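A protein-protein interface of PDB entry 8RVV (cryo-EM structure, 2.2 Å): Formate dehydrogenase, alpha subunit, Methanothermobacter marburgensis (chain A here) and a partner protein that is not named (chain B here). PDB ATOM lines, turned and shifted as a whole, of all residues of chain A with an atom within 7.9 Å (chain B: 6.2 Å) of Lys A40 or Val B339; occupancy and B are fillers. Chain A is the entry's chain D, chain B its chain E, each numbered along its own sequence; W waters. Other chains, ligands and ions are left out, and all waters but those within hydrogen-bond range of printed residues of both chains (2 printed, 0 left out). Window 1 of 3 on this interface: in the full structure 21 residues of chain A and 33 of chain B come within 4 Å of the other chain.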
ATOM      1  N   CYS A  14      17.742   8.108  32.432  1.00  0.00           N
ATOM      2  CA  CYS A  14      18.134   8.157  31.029  1.00  0.00           C
ATOM      3  C   CYS A  14      19.408   7.359  30.785  1.00  0.00           C
ATOM      4  O   CYS A  14      20.366   7.428  31.559  1.00  0.00           O
ATOM      5  CB  CYS A  14      18.337   9.604  30.585  1.00  0.00           C
ATOM      6  SG  CYS A  14      16.861  10.626  30.699  1.00  0.00           S
ATOM      7  N   GLY A  15      19.415   6.600  29.695  1.00  0.00           N
ATOM      8  CA  GLY A  15      20.585   5.848  29.274  1.00  0.00           C
ATOM      9  C   GLY A  15      21.386   6.622  28.243  1.00  0.00           C
ATOM     10  O   GLY A  15      20.825   7.328  27.405  1.00  0.00           O
ATOM     11  N   VAL A  16      22.709   6.486  28.319  1.00  0.00           N
ATOM     12  CA  VAL A  16      23.637   7.121  27.390  1.00  0.00           C
ATOM     13  C   VAL A  16      24.674   6.083  26.984  1.00  0.00           C
ATOM     14  O   VAL A  16      24.787   5.022  27.598  1.00  0.00           O
ATOM     15  CB  VAL A  16      24.316   8.366  28.003  1.00  0.00           C
ATOM     16  CG1 VAL A  16      23.273   9.352  28.478  1.00  0.00           C
ATOM     17  CG2 VAL A  16      25.222   7.976  29.156  1.00  0.00           C
ATOM     18  N   TYR A  29      27.314   8.897  22.861  1.00  0.00           N
ATOM     19  CA  TYR A  29      26.536   8.410  21.737  1.00  0.00           C
ATOM     20  C   TYR A  29      25.106   8.125  22.176  1.00  0.00           C
ATOM     21  O   TYR A  29      24.865   7.757  23.335  1.00  0.00           O
ATOM     22  CB  TYR A  29      27.167   7.141  21.139  1.00  0.00           C
ATOM     23  CG  TYR A  29      26.850   6.918  19.680  1.00  0.00           C
ATOM     24  CD1 TYR A  29      27.401   7.726  18.698  1.00  0.00           C
ATOM     25  CD2 TYR A  29      26.001   5.894  19.285  1.00  0.00           C
ATOM     26  CE1 TYR A  29      27.114   7.527  17.364  1.00  0.00           C
ATOM     27  CE2 TYR A  29      25.708   5.685  17.954  1.00  0.00           C
ATOM     28  CZ  TYR A  29      26.268   6.503  16.998  1.00  0.00           C
ATOM     29  OH  TYR A  29      25.980   6.299  15.670  1.00  0.00           O
ATOM     30  N   PRO A  30      24.130   8.299  21.277  1.00  0.00           N
ATOM     31  CA  PRO A  30      22.728   8.081  21.663  1.00  0.00           C
ATOM     32  C   PRO A  30      22.442   6.621  21.975  1.00  0.00           C
ATOM     33  O   PRO A  30      22.822   5.721  21.225  1.00  0.00           O
ATOM     34  CB  PRO A  30      21.940   8.555  20.435  1.00  0.00           C
ATOM     35  CG  PRO A  30      22.852   9.458  19.721  1.00  0.00           C
ATOM     36  CD  PRO A  30      24.226   8.914  19.943  1.00  0.00           C
ATOM     37  N   TYR A  31      21.756   6.397  23.095  1.00  0.00           N
ATOM     38  CA  TYR A  31      21.333   5.066  23.522  1.00  0.00           C
ATOM     39  C   TYR A  31      19.855   4.919  23.156  1.00  0.00           C
ATOM     40  O   TYR A  31      18.961   4.991  23.996  1.00  0.00           O
ATOM     41  CB  TYR A  31      21.600   4.899  25.018  1.00  0.00           C
ATOM     42  CG  TYR A  31      21.393   3.514  25.590  1.00  0.00           C
ATOM     43  CD1 TYR A  31      20.841   2.490  24.835  1.00  0.00           C
ATOM     44  CD2 TYR A  31      21.744   3.239  26.902  1.00  0.00           C
ATOM     45  CE1 TYR A  31      20.650   1.236  25.369  1.00  0.00           C
ATOM     46  CE2 TYR A  31      21.555   1.991  27.446  1.00  0.00           C
ATOM     47  CZ  TYR A  31      21.008   0.992  26.674  1.00  0.00           C
ATOM     48  OH  TYR A  31      20.822  -0.255  27.214  1.00  0.00           O
ATOM     49  N   ARG A  32      19.608   4.695  21.862  1.00  0.00           N
ATOM     50  CA  ARG A  32      18.248   4.751  21.332  1.00  0.00           C
ATOM     51  C   ARG A  32      17.356   3.664  21.917  1.00  0.00           C
ATOM     52  O   ARG A  32      16.135   3.837  21.987  1.00  0.00           O
ATOM     53  CB  ARG A  32      18.277   4.631  19.808  1.00  0.00           C
ATOM     54  CG  ARG A  32      18.542   5.936  19.086  1.00  0.00           C
ATOM     55  CD  ARG A  32      18.488   5.763  17.577  1.00  0.00           C
ATOM     56  NE  ARG A  32      18.786   7.006  16.877  1.00  0.00           N
ATOM     57  CZ  ARG A  32      20.007   7.433  16.580  1.00  0.00           C
ATOM     58  NH1 ARG A  32      21.083   6.729  16.894  1.00  0.00           N
ATOM     59  NH2 ARG A  32      20.153   8.597  15.956  1.00  0.00           N
ATOM     60  N   ARG A  33      17.940   2.541  22.332  1.00  0.00           N
ATOM     61  CA  ARG A  33      17.163   1.406  22.809  1.00  0.00           C
ATOM     62  C   ARG A  33      16.619   1.605  24.219  1.00  0.00           C
ATOM     63  O   ARG A  33      15.670   0.913  24.600  1.00  0.00           O
ATOM     64  CB  ARG A  33      18.028   0.144  22.754  1.00  0.00           C
ATOM     65  CG  ARG A  33      17.371  -1.121  23.275  1.00  0.00           C
ATOM     66  CD  ARG A  33      16.127  -1.485  22.485  1.00  0.00           C
ATOM     67  NE  ARG A  33      15.624  -2.804  22.847  1.00  0.00           N
ATOM     68  CZ  ARG A  33      15.052  -3.097  24.006  1.00  0.00           C
ATOM     69  NH1 ARG A  33      14.881  -2.182  24.945  1.00  0.00           N
ATOM     70  NH2 ARG A  33      14.644  -4.342  24.230  1.00  0.00           N
ATOM     71  N   HIS A  34      17.177   2.527  24.992  1.00  0.00           N
ATOM     72  CA  HIS A  34      16.746   2.685  26.373  1.00  0.00           C
ATOM     73  C   HIS A  34      15.302   3.188  26.425  1.00  0.00           C
ATOM     74  O   HIS A  34      14.940   4.111  25.693  1.00  0.00           O
ATOM     75  CB  HIS A  34      17.662   3.655  27.110  1.00  0.00           C
ATOM     76  CG  HIS A  34      17.641   3.489  28.596  1.00  0.00           C
ATOM     77  ND1 HIS A  34      16.672   4.055  29.394  1.00  0.00           N
ATOM     78  CD2 HIS A  34      18.472   2.825  29.432  1.00  0.00           C
ATOM     79  CE1 HIS A  34      16.902   3.742  30.655  1.00  0.00           C
ATOM     80  NE2 HIS A  34      17.990   2.997  30.705  1.00  0.00           N
ATOM     81  N   VAL A  36      13.536   4.718  28.908  1.00  0.00           N
ATOM     82  CA  VAL A  36      13.237   5.946  29.636  1.00  0.00           C
ATOM     83  C   VAL A  36      13.284   7.150  28.702  1.00  0.00           C
ATOM     84  O   VAL A  36      12.407   8.020  28.746  1.00  0.00           O
ATOM     85  CB  VAL A  36      14.201   6.114  30.826  1.00  0.00           C
ATOM     86  CG1 VAL A  36      14.235   7.560  31.292  1.00  0.00           C
ATOM     87  CG2 VAL A  36      13.794   5.198  31.968  1.00  0.00           C
ATOM     88  N   ASN A  37      14.305   7.223  27.846  1.00  0.00           N
ATOM     89  CA  ASN A  37      14.524   8.400  27.018  1.00  0.00           C
ATOM     90  C   ASN A  37      14.702   8.109  25.534  1.00  0.00           C
ATOM     91  O   ASN A  37      14.700   9.056  24.744  1.00  0.00           O
ATOM     92  CB  ASN A  37      15.749   9.180  27.518  1.00  0.00           C
ATOM     93  CG  ASN A  37      17.023   8.352  27.503  1.00  0.00           C
ATOM     94  OD1 ASN A  37      17.022   7.182  27.872  1.00  0.00           O
ATOM     95  ND2 ASN A  37      18.117   8.966  27.081  1.00  0.00           N
ATOM     96  N   GLU A  38      14.845   6.847  25.130  1.00  0.00           N
ATOM     97  CA  GLU A  38      14.940   6.473  23.718  1.00  0.00           C
ATOM     98  C   GLU A  38      16.038   7.252  22.998  1.00  0.00           C
ATOM     99  O   GLU A  38      15.872   7.678  21.854  1.00  0.00           O
ATOM    100  CB  GLU A  38      13.599   6.665  23.006  1.00  0.00           C
ATOM    101  CG  GLU A  38      12.381   6.480  23.893  1.00  0.00           C
ATOM    102  CD  GLU A  38      11.103   6.285  23.098  1.00  0.00           C
ATOM    103  OE1 GLU A  38      11.175   5.764  21.966  1.00  0.00           O
ATOM    104  OE2 GLU A  38      10.026   6.656  23.606  1.00  0.00           O
ATOM    105  N   GLY A  39      17.174   7.435  23.662  1.00  0.00           N
ATOM    106  CA  GLY A  39      18.306   8.090  23.046  1.00  0.00           C
ATOM    107  C   GLY A  39      18.274   9.600  23.074  1.00  0.00           C
ATOM    108  O   GLY A  39      19.170  10.229  22.501  1.00  0.00           O
ATOM    109  N   LYS A  40      17.277  10.203  23.708  1.00  0.00           N
ATOM    110  CA  LYS A  40      17.203  11.648  23.863  1.00  0.00           C
ATOM    111  C   LYS A  40      17.792  12.027  25.212  1.00  0.00           C
ATOM    112  O   LYS A  40      17.502  11.384  26.222  1.00  0.00           O
ATOM    113  CB  LYS A  40      15.757  12.135  23.755  1.00  0.00           C
ATOM    114  CG  LYS A  40      15.054  11.703  22.483  1.00  0.00           C
ATOM    115  CD  LYS A  40      13.545  11.812  22.599  1.00  0.00           C
ATOM    116  CE  LYS A  40      12.860  11.414  21.304  1.00  0.00           C
ATOM    117  NZ  LYS A  40      13.012  12.439  20.236  1.00  0.00           N
ATOM    118  N   THR A  41      18.631  13.056  25.224  1.00  0.00           N
ATOM    119  CA  THR A  41      19.244  13.523  26.455  1.00  0.00           C
ATOM    120  C   THR A  41      19.250  15.038  26.473  1.00  0.00           C
ATOM    121  O   THR A  41      19.281  15.687  25.426  1.00  0.00           O
ATOM    122  CB  THR A  41      20.683  13.009  26.618  1.00  0.00           C
ATOM    123  OG1 THR A  41      21.389  13.143  25.380  1.00  0.00           O
ATOM    124  CG2 THR A  41      20.699  11.558  27.055  1.00  0.00           C
ATOM    125  N   CYS A  42      19.207  15.595  27.678  1.00  0.00           N
ATOM    126  CA  CYS A  42      19.473  17.008  27.869  1.00  0.00           C
ATOM    127  C   CYS A  42      20.983  17.240  27.818  1.00  0.00           C
ATOM    128  O   CYS A  42      21.768  16.321  27.580  1.00  0.00           O
ATOM    129  CB  CYS A  42      18.862  17.485  29.186  1.00  0.00           C
ATOM    130  SG  CYS A  42      19.738  16.949  30.662  1.00  0.00           S
ATOM    131  N   GLY A  45      23.246  15.112  30.178  1.00  0.00           N
ATOM    132  CA  GLY A  45      23.435  13.741  29.739  1.00  0.00           C
ATOM    133  C   GLY A  45      24.542  13.607  28.713  1.00  0.00           C
ATOM    134  O   GLY A  45      25.288  12.626  28.716  1.00  0.00           O
ATOM    135  N   ARG A  46      24.662  14.585  27.819  1.00  0.00           N
ATOM    136  CA  ARG A  46      25.719  14.554  26.820  1.00  0.00           C
ATOM    137  C   ARG A  46      27.057  15.032  27.372  1.00  0.00           C
ATOM    138  O   ARG A  46      28.093  14.773  26.755  1.00  0.00           O
ATOM    139  CB  ARG A  46      25.310  15.397  25.610  1.00  0.00           C
ATOM    140  CG  ARG A  46      24.645  14.578  24.517  1.00  0.00           C
ATOM    141  CD  ARG A  46      23.866  15.430  23.535  1.00  0.00           C
ATOM    142  NE  ARG A  46      22.632  15.956  24.110  1.00  0.00           N
ATOM    143  CZ  ARG A  46      22.369  17.242  24.313  1.00  0.00           C
ATOM    144  NH1 ARG A  46      23.251  18.187  24.032  1.00  0.00           N
ATOM    145  NH2 ARG A  46      21.188  17.589  24.810  1.00  0.00           N
ATOM    146  N   PRO A 153      14.306  16.970  32.578  1.00  0.00           N
ATOM    147  CA  PRO A 153      13.729  17.251  31.254  1.00  0.00           C
ATOM    148  C   PRO A 153      13.025  16.066  30.614  1.00  0.00           C
ATOM    149  O   PRO A 153      12.011  16.254  29.929  1.00  0.00           O
ATOM    150  CB  PRO A 153      14.951  17.689  30.444  1.00  0.00           C
ATOM    151  CG  PRO A 153      15.842  18.313  31.442  1.00  0.00           C
ATOM    152  CD  PRO A 153      15.648  17.559  32.724  1.00  0.00           C
ATOM    153  N   LEU A 154      13.521  14.848  30.814  1.00  0.00           N
ATOM    154  CA  LEU A 154      12.927  13.699  30.148  1.00  0.00           C
ATOM    155  C   LEU A 154      11.698  13.159  30.876  1.00  0.00           C
ATOM    156  O   LEU A 154      11.041  12.255  30.353  1.00  0.00           O
ATOM    157  CB  LEU A 154      13.974  12.596  29.972  1.00  0.00           C
ATOM    158  CG  LEU A 154      14.767  12.607  28.655  1.00  0.00           C
ATOM    159  CD1 LEU A 154      13.858  12.469  27.443  1.00  0.00           C
ATOM    160  CD2 LEU A 154      15.636  13.853  28.522  1.00  0.00           C
ATOM    161  N   ARG A 157       9.175  15.755  29.345  1.00  0.00           N
ATOM    162  CA  ARG A 157       8.759  15.269  28.034  1.00  0.00           C
ATOM    163  C   ARG A 157       7.494  14.425  28.142  1.00  0.00           C
ATOM    164  O   ARG A 157       6.570  14.563  27.331  1.00  0.00           O
ATOM    165  CB  ARG A 157       9.900  14.467  27.402  1.00  0.00           C
ATOM    166  CG  ARG A 157       9.479  13.405  26.405  1.00  0.00           C
ATOM    167  CD  ARG A 157      10.696  12.767  25.765  1.00  0.00           C
ATOM    168  NE  ARG A 157      10.392  12.133  24.489  1.00  0.00           N
ATOM    169  CZ  ARG A 157      10.281  10.824  24.297  1.00  0.00           C
ATOM    170  NH1 ARG A 157      10.433   9.959  25.286  1.00  0.00           N
ATOM    171  NH2 ARG A 157      10.006  10.371  23.078  1.00  0.00           N
ATOM    172  N   ARG A 158       7.432  13.546  29.142  1.00  0.00           N
ATOM    173  CA  ARG A 158       6.232  12.743  29.338  1.00  0.00           C
ATOM    174  C   ARG A 158       5.062  13.602  29.795  1.00  0.00           C
ATOM    175  O   ARG A 158       3.914  13.312  29.452  1.00  0.00           O
ATOM    176  CB  ARG A 158       6.502  11.629  30.347  1.00  0.00           C
ATOM    177  CG  ARG A 158       7.702  10.767  30.010  1.00  0.00           C
ATOM    178  CD  ARG A 158       7.489   9.965  28.744  1.00  0.00           C
ATOM    179  NE  ARG A 158       8.587   9.038  28.506  1.00  0.00           N
ATOM    180  CZ  ARG A 158       8.586   8.092  27.579  1.00  0.00           C
ATOM    181  NH1 ARG A 158       7.548   7.904  26.784  1.00  0.00           N
ATOM    182  NH2 ARG A 158       9.655   7.313  27.448  1.00  0.00           N
ATOM    183  N   HIS A 161       3.700  14.842  26.679  1.00  0.00           N
ATOM    184  CA  HIS A 161       2.902  13.786  26.058  1.00  0.00           C
ATOM    185  C   HIS A 161       1.520  13.699  26.701  1.00  0.00           C
ATOM    186  O   HIS A 161       0.509  13.526  26.010  1.00  0.00           O
ATOM    187  CB  HIS A 161       3.620  12.440  26.172  1.00  0.00           C
ATOM    188  CG  HIS A 161       4.756  12.274  25.214  1.00  0.00           C
ATOM    189  ND1 HIS A 161       5.519  11.127  25.161  1.00  0.00           N
ATOM    190  CD2 HIS A 161       5.263  13.106  24.274  1.00  0.00           C
ATOM    191  CE1 HIS A 161       6.445  11.260  24.228  1.00  0.00           C
ATOM    192  NE2 HIS A 161       6.311  12.452  23.676  1.00  0.00           N
ATOM    193  N   CYS B 283      18.726  22.579  24.689  1.00  0.00           N
ATOM    194  CA  CYS B 283      19.679  21.551  25.077  1.00  0.00           C
ATOM    195  C   CYS B 283      20.760  21.303  24.037  1.00  0.00           C
ATOM    196  O   CYS B 283      21.775  20.682  24.361  1.00  0.00           O
ATOM    197  CB  CYS B 283      18.942  20.238  25.352  1.00  0.00           C
ATOM    198  SG  CYS B 283      18.344  19.403  23.878  1.00  0.00           S
ATOM    199  N   ALA B 285      20.786  19.303  21.600  1.00  0.00           N
ATOM    200  CA  ALA B 285      20.902  17.926  21.139  1.00  0.00           C
ATOM    201  C   ALA B 285      20.853  17.860  19.621  1.00  0.00           C
ATOM    202  O   ALA B 285      21.574  17.071  19.002  1.00  0.00           O
ATOM    203  CB  ALA B 285      19.797  17.066  21.750  1.00  0.00           C
ATOM    204  N   CYS B 286      20.009  18.688  19.004  1.00  0.00           N
ATOM    205  CA  CYS B 286      19.904  18.698  17.549  1.00  0.00           C
ATOM    206  C   CYS B 286      21.221  19.112  16.909  1.00  0.00           C
ATOM    207  O   CYS B 286      21.699  18.468  15.969  1.00  0.00           O
ATOM    208  CB  CYS B 286      18.774  19.630  17.113  1.00  0.00           C
ATOM    209  SG  CYS B 286      18.704  21.205  17.993  1.00  0.00           S
ATOM    210  N   ARG B 287      21.831  20.185  17.409  1.00  0.00           N
ATOM    211  CA  ARG B 287      23.097  20.635  16.847  1.00  0.00           C
ATOM    212  C   ARG B 287      24.200  19.608  17.078  1.00  0.00           C
ATOM    213  O   ARG B 287      25.004  19.345  16.179  1.00  0.00           O
ATOM    214  CB  ARG B 287      23.487  21.986  17.442  1.00  0.00           C
ATOM    215  CG  ARG B 287      24.713  22.601  16.784  1.00  0.00           C
ATOM    216  CD  ARG B 287      25.676  23.193  17.785  1.00  0.00           C
ATOM    217  NE  ARG B 287      25.976  22.306  18.900  1.00  0.00           N
ATOM    218  CZ  ARG B 287      26.283  22.722  20.121  1.00  0.00           C
ATOM    219  NH1 ARG B 287      26.379  24.009  20.408  1.00  0.00           N
ATOM    220  NH2 ARG B 287      26.496  21.827  21.079  1.00  0.00           N
ATOM    221  N   ALA B 289      23.874  16.382  17.370  1.00  0.00           N
ATOM    222  CA  ALA B 289      23.644  15.236  16.504  1.00  0.00           C
ATOM    223  C   ALA B 289      23.875  15.556  15.034  1.00  0.00           C
ATOM    224  O   ALA B 289      24.204  14.647  14.267  1.00  0.00           O
ATOM    225  CB  ALA B 289      22.223  14.709  16.701  1.00  0.00           C
ATOM    226  N   GLY B 334      17.868  13.192   9.551  1.00  0.00           N
ATOM    227  CA  GLY B 334      16.919  13.034  10.631  1.00  0.00           C
ATOM    228  C   GLY B 334      17.521  12.861  12.005  1.00  0.00           C
ATOM    229  O   GLY B 334      16.791  12.513  12.938  1.00  0.00           O
ATOM    230  N   GLN B 335      18.826  13.087  12.168  1.00  0.00           N
ATOM    231  CA  GLN B 335      19.446  12.887  13.473  1.00  0.00           C
ATOM    232  C   GLN B 335      19.012  13.961  14.464  1.00  0.00           C
ATOM    233  O   GLN B 335      18.870  13.683  15.659  1.00  0.00           O
ATOM    234  CB  GLN B 335      20.969  12.864  13.340  1.00  0.00           C
ATOM    235  CG  GLN B 335      21.500  11.738  12.470  1.00  0.00           C
ATOM    236  CD  GLN B 335      21.333  10.379  13.112  1.00  0.00           C
ATOM    237  OE1 GLN B 335      21.542  10.217  14.311  1.00  0.00           O
ATOM    238  NE2 GLN B 335      20.950   9.394  12.315  1.00  0.00           N
ATOM    239  N   CYS B 336      18.800  15.191  13.991  1.00  0.00           N
ATOM    240  CA  CYS B 336      18.347  16.254  14.879  1.00  0.00           C
ATOM    241  C   CYS B 336      16.992  15.922  15.489  1.00  0.00           C
ATOM    242  O   CYS B 336      16.769  16.136  16.684  1.00  0.00           O
ATOM    243  CB  CYS B 336      18.271  17.577  14.120  1.00  0.00           C
ATOM    244  SG  CYS B 336      17.425  17.465  12.526  1.00  0.00           S
ATOM    245  N   GLU B 337      16.074  15.399  14.678  1.00  0.00           N
ATOM    246  CA  GLU B 337      14.742  15.076  15.170  1.00  0.00           C
ATOM    247  C   GLU B 337      14.750  13.841  16.060  1.00  0.00           C
ATOM    248  O   GLU B 337      13.930  13.737  16.976  1.00  0.00           O
ATOM    249  CB  GLU B 337      13.790  14.873  13.994  1.00  0.00           C
ATOM    250  CG  GLU B 337      12.385  15.350  14.267  1.00  0.00           C
ATOM    251  CD  GLU B 337      11.409  14.961  13.179  1.00  0.00           C
ATOM    252  OE1 GLU B 337      11.554  15.457  12.041  1.00  0.00           O
ATOM    253  OE2 GLU B 337      10.490  14.168  13.465  1.00  0.00           O
ATOM    254  N   ASP B 338      15.661  12.901  15.809  1.00  0.00           N
ATOM    255  CA  ASP B 338      15.721  11.687  16.618  1.00  0.00           C
ATOM    256  C   ASP B 338      16.046  12.000  18.073  1.00  0.00           C
ATOM    257  O   ASP B 338      15.482  11.387  18.984  1.00  0.00           O
ATOM    258  CB  ASP B 338      16.766  10.730  16.046  1.00  0.00           C
ATOM    259  CG  ASP B 338      16.267   9.973  14.835  1.00  0.00           C
ATOM    260  OD1 ASP B 338      15.036   9.841  14.671  1.00  0.00           O
ATOM    261  OD2 ASP B 338      17.110   9.509  14.041  1.00  0.00           O
ATOM    262  N   VAL B 339      16.962  12.942  18.312  1.00  0.00           N
ATOM    263  CA  VAL B 339      17.504  13.144  19.651  1.00  0.00           C
ATOM    264  C   VAL B 339      16.811  14.262  20.410  1.00  0.00           C
ATOM    265  O   VAL B 339      17.156  14.508  21.572  1.00  0.00           O
ATOM    266  CB  VAL B 339      19.020  13.435  19.591  1.00  0.00           C
ATOM    267  CG1 VAL B 339      19.747  12.315  18.863  1.00  0.00           C
ATOM    268  CG2 VAL B 339      19.294  14.779  18.927  1.00  0.00           C
ATOM    269  N   CYS B 340      15.845  14.937  19.808  1.00  0.00           N
ATOM    270  CA  CYS B 340      15.230  16.085  20.457  1.00  0.00           C
ATOM    271  C   CYS B 340      14.438  15.634  21.681  1.00  0.00           C
ATOM    272  O   CYS B 340      13.484  14.860  21.536  1.00  0.00           O
ATOM    273  CB  CYS B 340      14.320  16.820  19.480  1.00  0.00           C
ATOM    274  SG  CYS B 340      13.562  18.301  20.162  1.00  0.00           S
ATOM    275  N   PRO B 341      14.777  16.093  22.891  1.00  0.00           N
ATOM    276  CA  PRO B 341      13.998  15.677  24.067  1.00  0.00           C
ATOM    277  C   PRO B 341      12.569  16.182  24.057  1.00  0.00           C
ATOM    278  O   PRO B 341      11.728  15.613  24.759  1.00  0.00           O
ATOM    279  CB  PRO B 341      14.782  16.267  25.251  1.00  0.00           C
ATOM    280  CG  PRO B 341      16.042  16.808  24.696  1.00  0.00           C
ATOM    281  CD  PRO B 341      15.848  17.038  23.244  1.00  0.00           C
ATOM    282  N   MET B 342      12.268  17.226  23.293  1.00  0.00           N
ATOM    283  CA  MET B 342      10.958  17.857  23.306  1.00  0.00           C
ATOM    284  C   MET B 342      10.080  17.427  22.137  1.00  0.00           C
ATOM    285  O   MET B 342       8.958  17.922  22.012  1.00  0.00           O
ATOM    286  CB  MET B 342      11.132  19.382  23.299  1.00  0.00           C
ATOM    287  CG  MET B 342      11.233  20.046  24.674  1.00  0.00           C
ATOM    288  SD  MET B 342      10.287  19.296  26.018  1.00  0.00           S
ATOM    289  CE  MET B 342      11.586  18.700  27.093  1.00  0.00           C
ATOM    290  N   ASP B 343      10.556  16.520  21.288  1.00  0.00           N
ATOM    291  CA  ASP B 343       9.778  15.975  20.176  1.00  0.00           C
ATOM    292  C   ASP B 343       9.322  17.075  19.210  1.00  0.00           C
ATOM    293  O   ASP B 343       8.138  17.222  18.907  1.00  0.00           O
ATOM    294  CB  ASP B 343       8.574  15.179  20.691  1.00  0.00           C
ATOM    295  CG  ASP B 343       8.975  13.932  21.445  1.00  0.00           C
ATOM    296  OD1 ASP B 343       9.498  12.991  20.818  1.00  0.00           O
ATOM    297  OD2 ASP B 343       8.752  13.889  22.669  1.00  0.00           O
HETATM  298  O   HOH W   1      23.552   7.983  15.482  1.00  0.00           O
HETATM  299  O   HOH W   2      15.601   7.282  16.556  1.00  0.00           O
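Tyr A31 touches none of the printed residues of chain B.
Of chain B, only Glu B337 (3.6 Å), Asp B338 (3.0 Å), Val B339 (3.5 Å), Cys B340 (2.8 Å), Pro B341 (3.97 Å) and Asp B343 (3.6 Å) come within 4 Å of Lys A40.
Of the printed residues of chain A, Gln B335 touches Arg A32.
Val B339 touches one residue of chain A.
Of the printed residues of chain A, Cys B340 touches Lys A40.
Of the printed residues of chain A, Met B342 touches Pro A153.
Of the printed residues of chain A, Asp B343 touches Lys A40, Arg A157 and His A161.
The nearest residue of chain A that does not touch Val B339 is Thr A41 (4.2 Å).
The nearest printed residue of chain A that does not touch Asp B343 is Arg A158 (6.6 Å).
The guanidinium group (NH2) of Arg A46 lies within hydrogen-bond range of the backbone carbonyl oxygen (O) of Thr A41 (2.8 Å).
OE2 of Glu A38 lies within salt-bridge range of NH1 of Arg A157, at 3.7 Å.
The guanidinium group (NH2) of Arg A46 sits close to the backbone carbonyl oxygen (O) of Cys A42 (3.1 Å).
N of Ala B285 lies close to SG of Cys B283 (3.3 Å).
N of Asp B343 sits close to SG of Cys B340 (3.7 Å).
The backbone NH (N) of Met B342 lies close to the side-chain sulfur (SG) of Cys B340 (3.6 Å).
Printed residues of chain A that touch a printed residue of chain B: Arg A32, Lys A40, Thr A41, Arg A46, Pro A153, Arg A157 and His A161.
Among the printed residues, 16 pairs touch across the chains.
NH2 of Arg A32 sits at hydrogen-bond distance from OE1 of Gln B335 (2.7 Å).
NH2 of Arg A32 is in salt-bridge range of OD2 of Asp B338 (3.7 Å).
NZ of Lys A40 is in hydrogen-bond range of O of Asp B338, at 3.0 Å.
O of Cys B340 lies within hydrogen-bond range of NZ of Lys A40, 2.8 Å away.
NE of Arg A157 is in salt-bridge range of OD2 of Asp B343 (3.0 Å).
The side-chain carboxylate of Asp B343 is in hydrogen-bond range of a ring nitrogen (NE2) of His A161 (3.0 Å).
O of Cys B283 lies within hydrogen-bond range of NH1 of Arg A46.
NZ of Lys A40 is in salt-bridge range of OD1 of Asp B343 (3.6 Å).
Among the printed residues, merely in contact across the chains: Lys A40 with Glu B337 (3.6 Å), Lys A40 with Val B339 (3.5 Å), Lys A40 with Pro B341 (3.97 Å), Thr A41 with Ala B285 (3.96 Å), Thr A41 with Pro B341 (3.5 Å), Arg A46 with Ala B285 (3.4 Å), Pro A153 with Met B342 (3.8 Å) and Arg A157 with Pro B341 (3.2 Å).
Water W1 lies within hydrogen-bond range of OH of Tyr A29, NH1 of Arg A32 and OE1 of Gln B335.
Water W2 bridges the guanidinium group (NE) of Arg A32 (3.2 Å) and the side-chain carboxylate (OD1) of Asp B338 (3.2 Å).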
